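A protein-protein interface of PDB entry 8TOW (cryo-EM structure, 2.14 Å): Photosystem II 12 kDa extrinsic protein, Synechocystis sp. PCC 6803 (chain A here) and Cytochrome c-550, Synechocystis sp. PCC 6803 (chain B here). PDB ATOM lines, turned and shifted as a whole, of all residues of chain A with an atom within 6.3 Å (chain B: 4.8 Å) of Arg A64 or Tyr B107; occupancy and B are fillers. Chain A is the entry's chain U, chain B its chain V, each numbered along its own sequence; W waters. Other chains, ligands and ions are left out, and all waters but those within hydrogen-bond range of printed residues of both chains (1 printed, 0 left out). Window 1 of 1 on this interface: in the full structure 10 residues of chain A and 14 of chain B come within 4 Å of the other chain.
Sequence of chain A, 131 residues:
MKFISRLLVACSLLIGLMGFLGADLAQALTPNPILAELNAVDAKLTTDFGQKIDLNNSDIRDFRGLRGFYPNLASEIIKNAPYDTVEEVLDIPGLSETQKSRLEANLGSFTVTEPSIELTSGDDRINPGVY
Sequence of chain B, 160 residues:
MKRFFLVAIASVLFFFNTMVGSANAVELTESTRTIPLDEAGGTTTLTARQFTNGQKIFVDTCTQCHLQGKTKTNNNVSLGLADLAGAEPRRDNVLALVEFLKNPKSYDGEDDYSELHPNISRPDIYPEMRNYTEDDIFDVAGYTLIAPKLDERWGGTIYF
The guanidinium group (NH1) of Arg A61 sits at hydrogen-bond distance from the side-chain amide oxygen (OD1) of Asn B76 (2.9 Å). The guanidinium group (NH1) of Arg A64 is in hydrogen-bond range of the backbone carbonyl oxygen (O) of Asn B76 (2.7 Å). The guanidinium group of Arg A67 sits at hydrogen-bond distance from the backbone carbonyl oxygen of Ala B87 (2.6 Å). ND2 of Asn B76 sits at hydrogen-bond distance from OH of Tyr A70. The backbone carbonyl oxygen (O) of Tyr A70 is in hydrogen-bond range of the backbone NH (N) of Asp B108 (2.9 Å). N of Pro A71 sits close to OD2 of Asp B108, at 3.2 Å.
NE of Arg A64 sits at hydrogen-bond distance from O of Arg A61 (2.8 Å). OH of Tyr B107 lies within hydrogen-bond range of N of Ala B87. The backbone NH (N) of Glu B88 is in hydrogen-bond range of the backbone carbonyl oxygen (O) of Tyr B107 (2.9 Å). N of Gly B109 sits close to O of Glu B88. The side-chain carboxylate (OD1) of Asp B108 sits at hydrogen-bond distance from the side-chain hydroxyl (OG) of Ser B106 (2.6 Å).
Among the printed residues, pairs that only touch across the chains: Tyr A70 with Tyr B107, Arg A67 with Glu B88, Arg A67 with Gly B86, Gly A68 with Asp B108, Phe A69 with Asp B108, Arg A61 with Asn B75, Tyr A70 with Val B77, Gly A68 with Glu B88, Arg A64 with Tyr B107 and Arg A64 with Gly B86.
Of chain B, only Asn B76, Gly B86 and Tyr B107 come within 4 Å of Arg A64. Of the printed residues of chain B, Phe A69 touches Asp B108. Of the printed residues of chain A, Glu B88 touches Arg A67 (3.3 Å) and Gly A68 (3.9 Å). Printed residues of chain A within 4 Å of Val B77: Tyr A70. Printed residues of chain A within 4 Å of Asp B108: Gly A68, Phe A69, Tyr A70 and Pro A71. Of the printed residues of chain B, Pro A71 touches Asp B108. The nearest printed residue of chain A that does not touch Ala B87 is Gly A68 (5.4 Å).
Printed residues of chain A that touch a printed residue of chain B: Arg A61, Arg A64, Arg A67, Gly A68, Phe A69, Tyr A70 and Pro A71. Of the 15 printed residues of chain B, 8 touch a printed residue of chain A. Hydrophobic or aromatic side chains of chain B within 4 Å of the printed part of chain A: Val B77 and Tyr B107. Among the printed residues, 16 pairs touch across the chains.
Water W1 lies within hydrogen-bond range of the backbone carbonyl oxygen (O) of Gly B86 (2.7 Å), the backbone NH (N) of Gly A68 (3.1 Å) and the backbone carbonyl oxygen (O) of Tyr B107 (3.2 Å).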
ATOM      1  N   ILE A  60       6.736  -3.990 -15.116  1.00  0.00           N
ATOM      2  CA  ILE A  60       6.885  -3.184 -16.321  1.00  0.00           C
ATOM      3  C   ILE A  60       5.532  -2.663 -16.804  1.00  0.00           C
ATOM      4  O   ILE A  60       5.447  -1.552 -17.351  1.00  0.00           O
ATOM      5  CB  ILE A  60       7.646  -4.000 -17.391  1.00  0.00           C
ATOM      6  CG1 ILE A  60       8.084  -3.119 -18.556  1.00  0.00           C
ATOM      7  CG2 ILE A  60       6.876  -5.248 -17.843  1.00  0.00           C
ATOM      8  CD1 ILE A  60       9.509  -3.364 -18.977  1.00  0.00           C
ATOM      9  N   ARG A  61       4.452  -3.415 -16.551  1.00  0.00           N
ATOM     10  CA  ARG A  61       3.107  -3.015 -16.947  1.00  0.00           C
ATOM     11  C   ARG A  61       2.629  -1.767 -16.225  1.00  0.00           C
ATOM     12  O   ARG A  61       1.740  -1.075 -16.729  1.00  0.00           O
ATOM     13  CB  ARG A  61       2.118  -4.146 -16.679  1.00  0.00           C
ATOM     14  CG  ARG A  61       2.054  -5.196 -17.763  1.00  0.00           C
ATOM     15  CD  ARG A  61       1.446  -6.479 -17.218  1.00  0.00           C
ATOM     16  NE  ARG A  61       0.057  -6.303 -16.812  1.00  0.00           N
ATOM     17  CZ  ARG A  61      -0.982  -6.339 -17.637  1.00  0.00           C
ATOM     18  NH1 ARG A  61      -0.826  -6.515 -18.938  1.00  0.00           N
ATOM     19  NH2 ARG A  61      -2.207  -6.198 -17.141  1.00  0.00           N
ATOM     20  N   ASP A  62       3.199  -1.465 -15.060  1.00  0.00           N
ATOM     21  CA  ASP A  62       2.852  -0.243 -14.351  1.00  0.00           C
ATOM     22  C   ASP A  62       3.416   1.001 -15.020  1.00  0.00           C
ATOM     23  O   ASP A  62       2.987   2.108 -14.687  1.00  0.00           O
ATOM     24  CB  ASP A  62       3.335  -0.322 -12.905  1.00  0.00           C
ATOM     25  CG  ASP A  62       2.641  -1.415 -12.119  1.00  0.00           C
ATOM     26  OD1 ASP A  62       1.550  -1.152 -11.575  1.00  0.00           O
ATOM     27  OD2 ASP A  62       3.187  -2.533 -12.037  1.00  0.00           O
ATOM     28  N   PHE A  63       4.344   0.854 -15.966  1.00  0.00           N
ATOM     29  CA  PHE A  63       4.909   2.012 -16.643  1.00  0.00           C
ATOM     30  C   PHE A  63       4.128   2.427 -17.883  1.00  0.00           C
ATOM     31  O   PHE A  63       4.523   3.389 -18.548  1.00  0.00           O
ATOM     32  CB  PHE A  63       6.361   1.738 -17.024  1.00  0.00           C
ATOM     33  CG  PHE A  63       7.300   1.717 -15.855  1.00  0.00           C
ATOM     34  CD1 PHE A  63       7.520   0.546 -15.143  1.00  0.00           C
ATOM     35  CD2 PHE A  63       7.960   2.868 -15.463  1.00  0.00           C
ATOM     36  CE1 PHE A  63       8.378   0.528 -14.065  1.00  0.00           C
ATOM     37  CE2 PHE A  63       8.821   2.856 -14.378  1.00  0.00           C
ATOM     38  CZ  PHE A  63       9.034   1.686 -13.686  1.00  0.00           C
ATOM     39  N   ARG A  64       3.030   1.736 -18.199  1.00  0.00           N
ATOM     40  CA  ARG A  64       2.298   2.012 -19.432  1.00  0.00           C
ATOM     41  C   ARG A  64       1.511   3.314 -19.357  1.00  0.00           C
ATOM     42  O   ARG A  64       1.275   3.948 -20.390  1.00  0.00           O
ATOM     43  CB  ARG A  64       1.368   0.843 -19.752  1.00  0.00           C
ATOM     44  CG  ARG A  64       2.047  -0.254 -20.529  1.00  0.00           C
ATOM     45  CD  ARG A  64       1.297  -1.572 -20.470  1.00  0.00           C
ATOM     46  NE  ARG A  64       0.654  -1.847 -19.192  1.00  0.00           N
ATOM     47  CZ  ARG A  64      -0.478  -2.526 -19.068  1.00  0.00           C
ATOM     48  NH1 ARG A  64      -1.150  -2.946 -20.127  1.00  0.00           N
ATOM     49  NH2 ARG A  64      -0.945  -2.798 -17.853  1.00  0.00           N
ATOM     50  N   GLY A  65       1.110   3.735 -18.155  1.00  0.00           N
ATOM     51  CA  GLY A  65       0.417   5.003 -18.002  1.00  0.00           C
ATOM     52  C   GLY A  65       1.298   6.211 -18.234  1.00  0.00           C
ATOM     53  O   GLY A  65       0.781   7.311 -18.460  1.00  0.00           O
ATOM     54  N   LEU A  66       2.612   6.029 -18.181  1.00  0.00           N
ATOM     55  CA  LEU A  66       3.572   7.083 -18.472  1.00  0.00           C
ATOM     56  C   LEU A  66       3.883   7.004 -19.955  1.00  0.00           C
ATOM     57  O   LEU A  66       4.348   5.967 -20.438  1.00  0.00           O
ATOM     58  CB  LEU A  66       4.838   6.900 -17.647  1.00  0.00           C
ATOM     59  CG  LEU A  66       4.835   7.249 -16.173  1.00  0.00           C
ATOM     60  CD1 LEU A  66       4.491   6.021 -15.440  1.00  0.00           C
ATOM     61  CD2 LEU A  66       6.202   7.638 -15.788  1.00  0.00           C
ATOM     62  N   ARG A  67       3.615   8.086 -20.676  1.00  0.00           N
ATOM     63  CA  ARG A  67       3.761   8.081 -22.124  1.00  0.00           C
ATOM     64  C   ARG A  67       5.232   8.003 -22.517  1.00  0.00           C
ATOM     65  O   ARG A  67       6.077   8.694 -21.943  1.00  0.00           O
ATOM     66  CB  ARG A  67       3.121   9.330 -22.716  1.00  0.00           C
ATOM     67  CG  ARG A  67       3.119   9.363 -24.227  1.00  0.00           C
ATOM     68  CD  ARG A  67       2.147  10.398 -24.758  1.00  0.00           C
ATOM     69  NE  ARG A  67       0.996  10.569 -23.882  1.00  0.00           N
ATOM     70  CZ  ARG A  67      -0.122   9.863 -23.971  1.00  0.00           C
ATOM     71  NH1 ARG A  67      -0.263   8.903 -24.870  1.00  0.00           N
ATOM     72  NH2 ARG A  67      -1.119  10.120 -23.130  1.00  0.00           N
ATOM     73  N   GLY A  68       5.534   7.142 -23.484  1.00  0.00           N
ATOM     74  CA  GLY A  68       6.884   6.996 -23.976  1.00  0.00           C
ATOM     75  C   GLY A  68       7.795   6.139 -23.133  1.00  0.00           C
ATOM     76  O   GLY A  68       9.010   6.161 -23.347  1.00  0.00           O
ATOM     77  N   PHE A  69       7.254   5.389 -22.177  1.00  0.00           N
ATOM     78  CA  PHE A  69       8.054   4.554 -21.290  1.00  0.00           C
ATOM     79  C   PHE A  69       8.092   3.096 -21.709  1.00  0.00           C
ATOM     80  O   PHE A  69       9.176   2.547 -21.907  1.00  0.00           O
ATOM     81  CB  PHE A  69       7.523   4.647 -19.855  1.00  0.00           C
ATOM     82  CG  PHE A  69       8.167   5.729 -19.040  1.00  0.00           C
ATOM     83  CD1 PHE A  69       7.949   7.065 -19.344  1.00  0.00           C
ATOM     84  CD2 PHE A  69       8.992   5.413 -17.974  1.00  0.00           C
ATOM     85  CE1 PHE A  69       8.533   8.064 -18.594  1.00  0.00           C
ATOM     86  CE2 PHE A  69       9.582   6.407 -17.223  1.00  0.00           C
ATOM     87  CZ  PHE A  69       9.351   7.737 -17.533  1.00  0.00           C
ATOM     88  N   TYR A  70       6.942   2.466 -21.852  1.00  0.00           N
ATOM     89  CA  TYR A  70       6.832   1.068 -22.245  1.00  0.00           C
ATOM     90  C   TYR A  70       7.082   0.926 -23.742  1.00  0.00           C
ATOM     91  O   TYR A  70       6.460   1.638 -24.533  1.00  0.00           O
ATOM     92  CB  TYR A  70       5.454   0.513 -21.896  1.00  0.00           C
ATOM     93  CG  TYR A  70       5.345  -0.982 -22.079  1.00  0.00           C
ATOM     94  CD1 TYR A  70       5.733  -1.852 -21.068  1.00  0.00           C
ATOM     95  CD2 TYR A  70       4.862  -1.527 -23.266  1.00  0.00           C
ATOM     96  CE1 TYR A  70       5.643  -3.221 -21.234  1.00  0.00           C
ATOM     97  CE2 TYR A  70       4.777  -2.889 -23.441  1.00  0.00           C
ATOM     98  CZ  TYR A  70       5.167  -3.731 -22.423  1.00  0.00           C
ATOM     99  OH  TYR A  70       5.076  -5.091 -22.597  1.00  0.00           O
ATOM    100  N   PRO A  71       7.937  -0.011 -24.177  1.00  0.00           N
ATOM    101  CA  PRO A  71       8.672  -0.946 -23.326  1.00  0.00           C
ATOM    102  C   PRO A  71      10.143  -0.600 -23.066  1.00  0.00           C
ATOM    103  O   PRO A  71      10.708  -1.197 -22.164  1.00  0.00           O
ATOM    104  CB  PRO A  71       8.566  -2.249 -24.111  1.00  0.00           C
ATOM    105  CG  PRO A  71       8.569  -1.820 -25.525  1.00  0.00           C
ATOM    106  CD  PRO A  71       7.940  -0.454 -25.585  1.00  0.00           C
ATOM    107  N   ASN B  75      -0.599  -8.895 -24.259  1.00  0.00           N
ATOM    108  CA  ASN B  75      -1.739  -8.210 -23.657  1.00  0.00           C
ATOM    109  C   ASN B  75      -1.351  -6.994 -22.833  1.00  0.00           C
ATOM    110  O   ASN B  75      -2.242  -6.320 -22.305  1.00  0.00           O
ATOM    111  CB  ASN B  75      -2.567  -9.165 -22.798  1.00  0.00           C
ATOM    112  CG  ASN B  75      -4.046  -8.812 -22.821  1.00  0.00           C
ATOM    113  OD1 ASN B  75      -4.565  -8.379 -23.845  1.00  0.00           O
ATOM    114  ND2 ASN B  75      -4.720  -8.971 -21.696  1.00  0.00           N
ATOM    115  N   ASN B  76      -0.058  -6.697 -22.702  1.00  0.00           N
ATOM    116  CA  ASN B  76       0.338  -5.384 -22.210  1.00  0.00           C
ATOM    117  C   ASN B  76      -0.083  -4.285 -23.172  1.00  0.00           C
ATOM    118  O   ASN B  76      -0.376  -3.166 -22.747  1.00  0.00           O
ATOM    119  CB  ASN B  76       1.849  -5.334 -21.991  1.00  0.00           C
ATOM    120  CG  ASN B  76       2.336  -6.408 -21.044  1.00  0.00           C
ATOM    121  OD1 ASN B  76       1.544  -7.138 -20.454  1.00  0.00           O
ATOM    122  ND2 ASN B  76       3.647  -6.502 -20.887  1.00  0.00           N
ATOM    123  N   VAL B  77      -0.126  -4.584 -24.462  1.00  0.00           N
ATOM    124  CA  VAL B  77      -0.482  -3.614 -25.492  1.00  0.00           C
ATOM    125  C   VAL B  77      -1.762  -4.131 -26.140  1.00  0.00           C
ATOM    126  O   VAL B  77      -1.734  -4.850 -27.144  1.00  0.00           O
ATOM    127  CB  VAL B  77       0.641  -3.432 -26.515  1.00  0.00           C
ATOM    128  CG1 VAL B  77       0.346  -2.290 -27.454  1.00  0.00           C
ATOM    129  CG2 VAL B  77       1.969  -3.199 -25.810  1.00  0.00           C
ATOM    130  N   ALA B  82      -7.848   2.964 -23.022  1.00  0.00           N
ATOM    131  CA  ALA B  82      -6.752   3.435 -22.181  1.00  0.00           C
ATOM    132  C   ALA B  82      -5.404   3.016 -22.754  1.00  0.00           C
ATOM    133  O   ALA B  82      -4.432   3.784 -22.708  1.00  0.00           O
ATOM    134  CB  ALA B  82      -6.923   2.903 -20.757  1.00  0.00           C
ATOM    135  N   ASP B  83      -5.338   1.799 -23.303  1.00  0.00           N
ATOM    136  CA  ASP B  83      -4.135   1.327 -23.979  1.00  0.00           C
ATOM    137  C   ASP B  83      -3.822   2.176 -25.200  1.00  0.00           C
ATOM    138  O   ASP B  83      -2.665   2.539 -25.431  1.00  0.00           O
ATOM    139  CB  ASP B  83      -4.310  -0.133 -24.384  1.00  0.00           C
ATOM    140  CG  ASP B  83      -3.577  -1.085 -23.476  1.00  0.00           C
ATOM    141  OD1 ASP B  83      -2.379  -1.323 -23.725  1.00  0.00           O
ATOM    142  OD2 ASP B  83      -4.195  -1.607 -22.527  1.00  0.00           O
ATOM    143  N   LEU B  84      -4.847   2.507 -25.989  1.00  0.00           N
ATOM    144  CA  LEU B  84      -4.656   3.346 -27.167  1.00  0.00           C
ATOM    145  C   LEU B  84      -4.239   4.764 -26.792  1.00  0.00           C
ATOM    146  O   LEU B  84      -3.393   5.359 -27.468  1.00  0.00           O
ATOM    147  CB  LEU B  84      -5.941   3.363 -27.997  1.00  0.00           C
ATOM    148  CG  LEU B  84      -6.318   2.056 -28.703  1.00  0.00           C
ATOM    149  CD1 LEU B  84      -7.563   2.232 -29.554  1.00  0.00           C
ATOM    150  CD2 LEU B  84      -5.164   1.542 -29.543  1.00  0.00           C
ATOM    151  N   GLY B  86      -2.540   5.623 -24.074  1.00  0.00           N
ATOM    152  CA  GLY B  86      -1.228   5.673 -23.460  1.00  0.00           C
ATOM    153  C   GLY B  86      -0.045   5.490 -24.392  1.00  0.00           C
ATOM    154  O   GLY B  86       1.104   5.591 -23.955  1.00  0.00           O
ATOM    155  N   ALA B  87      -0.302   5.218 -25.671  1.00  0.00           N
ATOM    156  CA  ALA B  87       0.770   5.029 -26.643  1.00  0.00           C
ATOM    157  C   ALA B  87       1.460   6.348 -26.976  1.00  0.00           C
ATOM    158  O   ALA B  87       0.922   7.421 -26.691  1.00  0.00           O
ATOM    159  CB  ALA B  87       0.226   4.379 -27.915  1.00  0.00           C
ATOM    160  N   GLU B  88       2.659   6.280 -27.553  1.00  0.00           N
ATOM    161  CA  GLU B  88       3.399   7.469 -27.983  1.00  0.00           C
ATOM    162  C   GLU B  88       3.580   7.425 -29.496  1.00  0.00           C
ATOM    163  O   GLU B  88       4.296   6.550 -30.013  1.00  0.00           O
ATOM    164  CB  GLU B  88       4.749   7.577 -27.269  1.00  0.00           C
ATOM    165  CG  GLU B  88       5.781   8.508 -27.935  1.00  0.00           C
ATOM    166  CD  GLU B  88       5.604   9.980 -27.613  1.00  0.00           C
ATOM    167  OE1 GLU B  88       4.587  10.357 -26.999  1.00  0.00           O
ATOM    168  OE2 GLU B  88       6.506  10.768 -27.964  1.00  0.00           O
ATOM    169  N   ARG B  91      -3.029   6.702 -29.667  1.00  0.00           N
ATOM    170  CA  ARG B  91      -3.694   6.003 -30.757  1.00  0.00           C
ATOM    171  C   ARG B  91      -5.199   5.902 -30.539  1.00  0.00           C
ATOM    172  O   ARG B  91      -5.815   4.909 -30.933  1.00  0.00           O
ATOM    173  CB  ARG B  91      -3.079   4.614 -30.944  1.00  0.00           C
ATOM    174  CG  ARG B  91      -1.575   4.639 -31.187  1.00  0.00           C
ATOM    175  CD  ARG B  91      -0.970   3.247 -31.296  1.00  0.00           C
ATOM    176  NE  ARG B  91       0.453   3.300 -31.613  1.00  0.00           N
ATOM    177  CZ  ARG B  91       1.365   2.446 -31.168  1.00  0.00           C
ATOM    178  NH1 ARG B  91       1.036   1.415 -30.405  1.00  0.00           N
ATOM    179  NH2 ARG B  91       2.640   2.627 -31.501  1.00  0.00           N
ATOM    180  N   LYS B 105       4.799   0.803 -34.861  1.00  0.00           N
ATOM    181  CA  LYS B 105       5.943   1.038 -34.005  1.00  0.00           C
ATOM    182  C   LYS B 105       5.732   0.304 -32.691  1.00  0.00           C
ATOM    183  O   LYS B 105       4.734  -0.393 -32.492  1.00  0.00           O
ATOM    184  CB  LYS B 105       6.162   2.537 -33.764  1.00  0.00           C
ATOM    185  CG  LYS B 105       6.309   3.379 -35.025  1.00  0.00           C
ATOM    186  CD  LYS B 105       7.459   2.896 -35.897  1.00  0.00           C
ATOM    187  CE  LYS B 105       7.625   3.749 -37.152  1.00  0.00           C
ATOM    188  NZ  LYS B 105       6.917   5.059 -37.061  1.00  0.00           N
ATOM    189  N   SER B 106       6.678   0.485 -31.777  1.00  0.00           N
ATOM    190  CA  SER B 106       6.487   0.038 -30.410  1.00  0.00           C
ATOM    191  C   SER B 106       5.491   0.950 -29.695  1.00  0.00           C
ATOM    192  O   SER B 106       4.981   1.927 -30.253  1.00  0.00           O
ATOM    193  CB  SER B 106       7.820   0.004 -29.665  1.00  0.00           C
ATOM    194  OG  SER B 106       8.515   1.229 -29.809  1.00  0.00           O
ATOM    195  N   TYR B 107       5.210   0.610 -28.436  1.00  0.00           N
ATOM    196  CA  TYR B 107       4.247   1.382 -27.659  1.00  0.00           C
ATOM    197  C   TYR B 107       4.765   2.786 -27.368  1.00  0.00           C
ATOM    198  O   TYR B 107       3.994   3.751 -27.368  1.00  0.00           O
ATOM    199  CB  TYR B 107       3.918   0.651 -26.364  1.00  0.00           C
ATOM    200  CG  TYR B 107       2.660   1.142 -25.711  1.00  0.00           C
ATOM    201  CD1 TYR B 107       1.436   1.014 -26.352  1.00  0.00           C
ATOM    202  CD2 TYR B 107       2.691   1.737 -24.458  1.00  0.00           C
ATOM    203  CE1 TYR B 107       0.282   1.455 -25.762  1.00  0.00           C
ATOM    204  CE2 TYR B 107       1.535   2.191 -23.861  1.00  0.00           C
ATOM    205  CZ  TYR B 107       0.335   2.048 -24.520  1.00  0.00           C
ATOM    206  OH  TYR B 107      -0.826   2.483 -23.937  1.00  0.00           O
ATOM    207  N   ASP B 108       6.071   2.921 -27.141  1.00  0.00           N
ATOM    208  CA  ASP B 108       6.690   4.225 -26.960  1.00  0.00           C
ATOM    209  C   ASP B 108       7.075   4.877 -28.279  1.00  0.00           C
ATOM    210  O   ASP B 108       7.708   5.935 -28.265  1.00  0.00           O
ATOM    211  CB  ASP B 108       7.926   4.115 -26.062  1.00  0.00           C
ATOM    212  CG  ASP B 108       8.785   2.900 -26.373  1.00  0.00           C
ATOM    213  OD1 ASP B 108       8.717   2.375 -27.501  1.00  0.00           O
ATOM    214  OD2 ASP B 108       9.532   2.467 -25.476  1.00  0.00           O
ATOM    215  N   GLY B 109       6.763   4.246 -29.411  1.00  0.00           N
ATOM    216  CA  GLY B 109       7.063   4.822 -30.704  1.00  0.00           C
ATOM    217  C   GLY B 109       8.520   4.802 -31.101  1.00  0.00           C
ATOM    218  O   GLY B 109       8.888   5.429 -32.095  1.00  0.00           O
HETATM  219  O   HOH W   1       3.659   4.793 -24.407  1.00  0.00           O
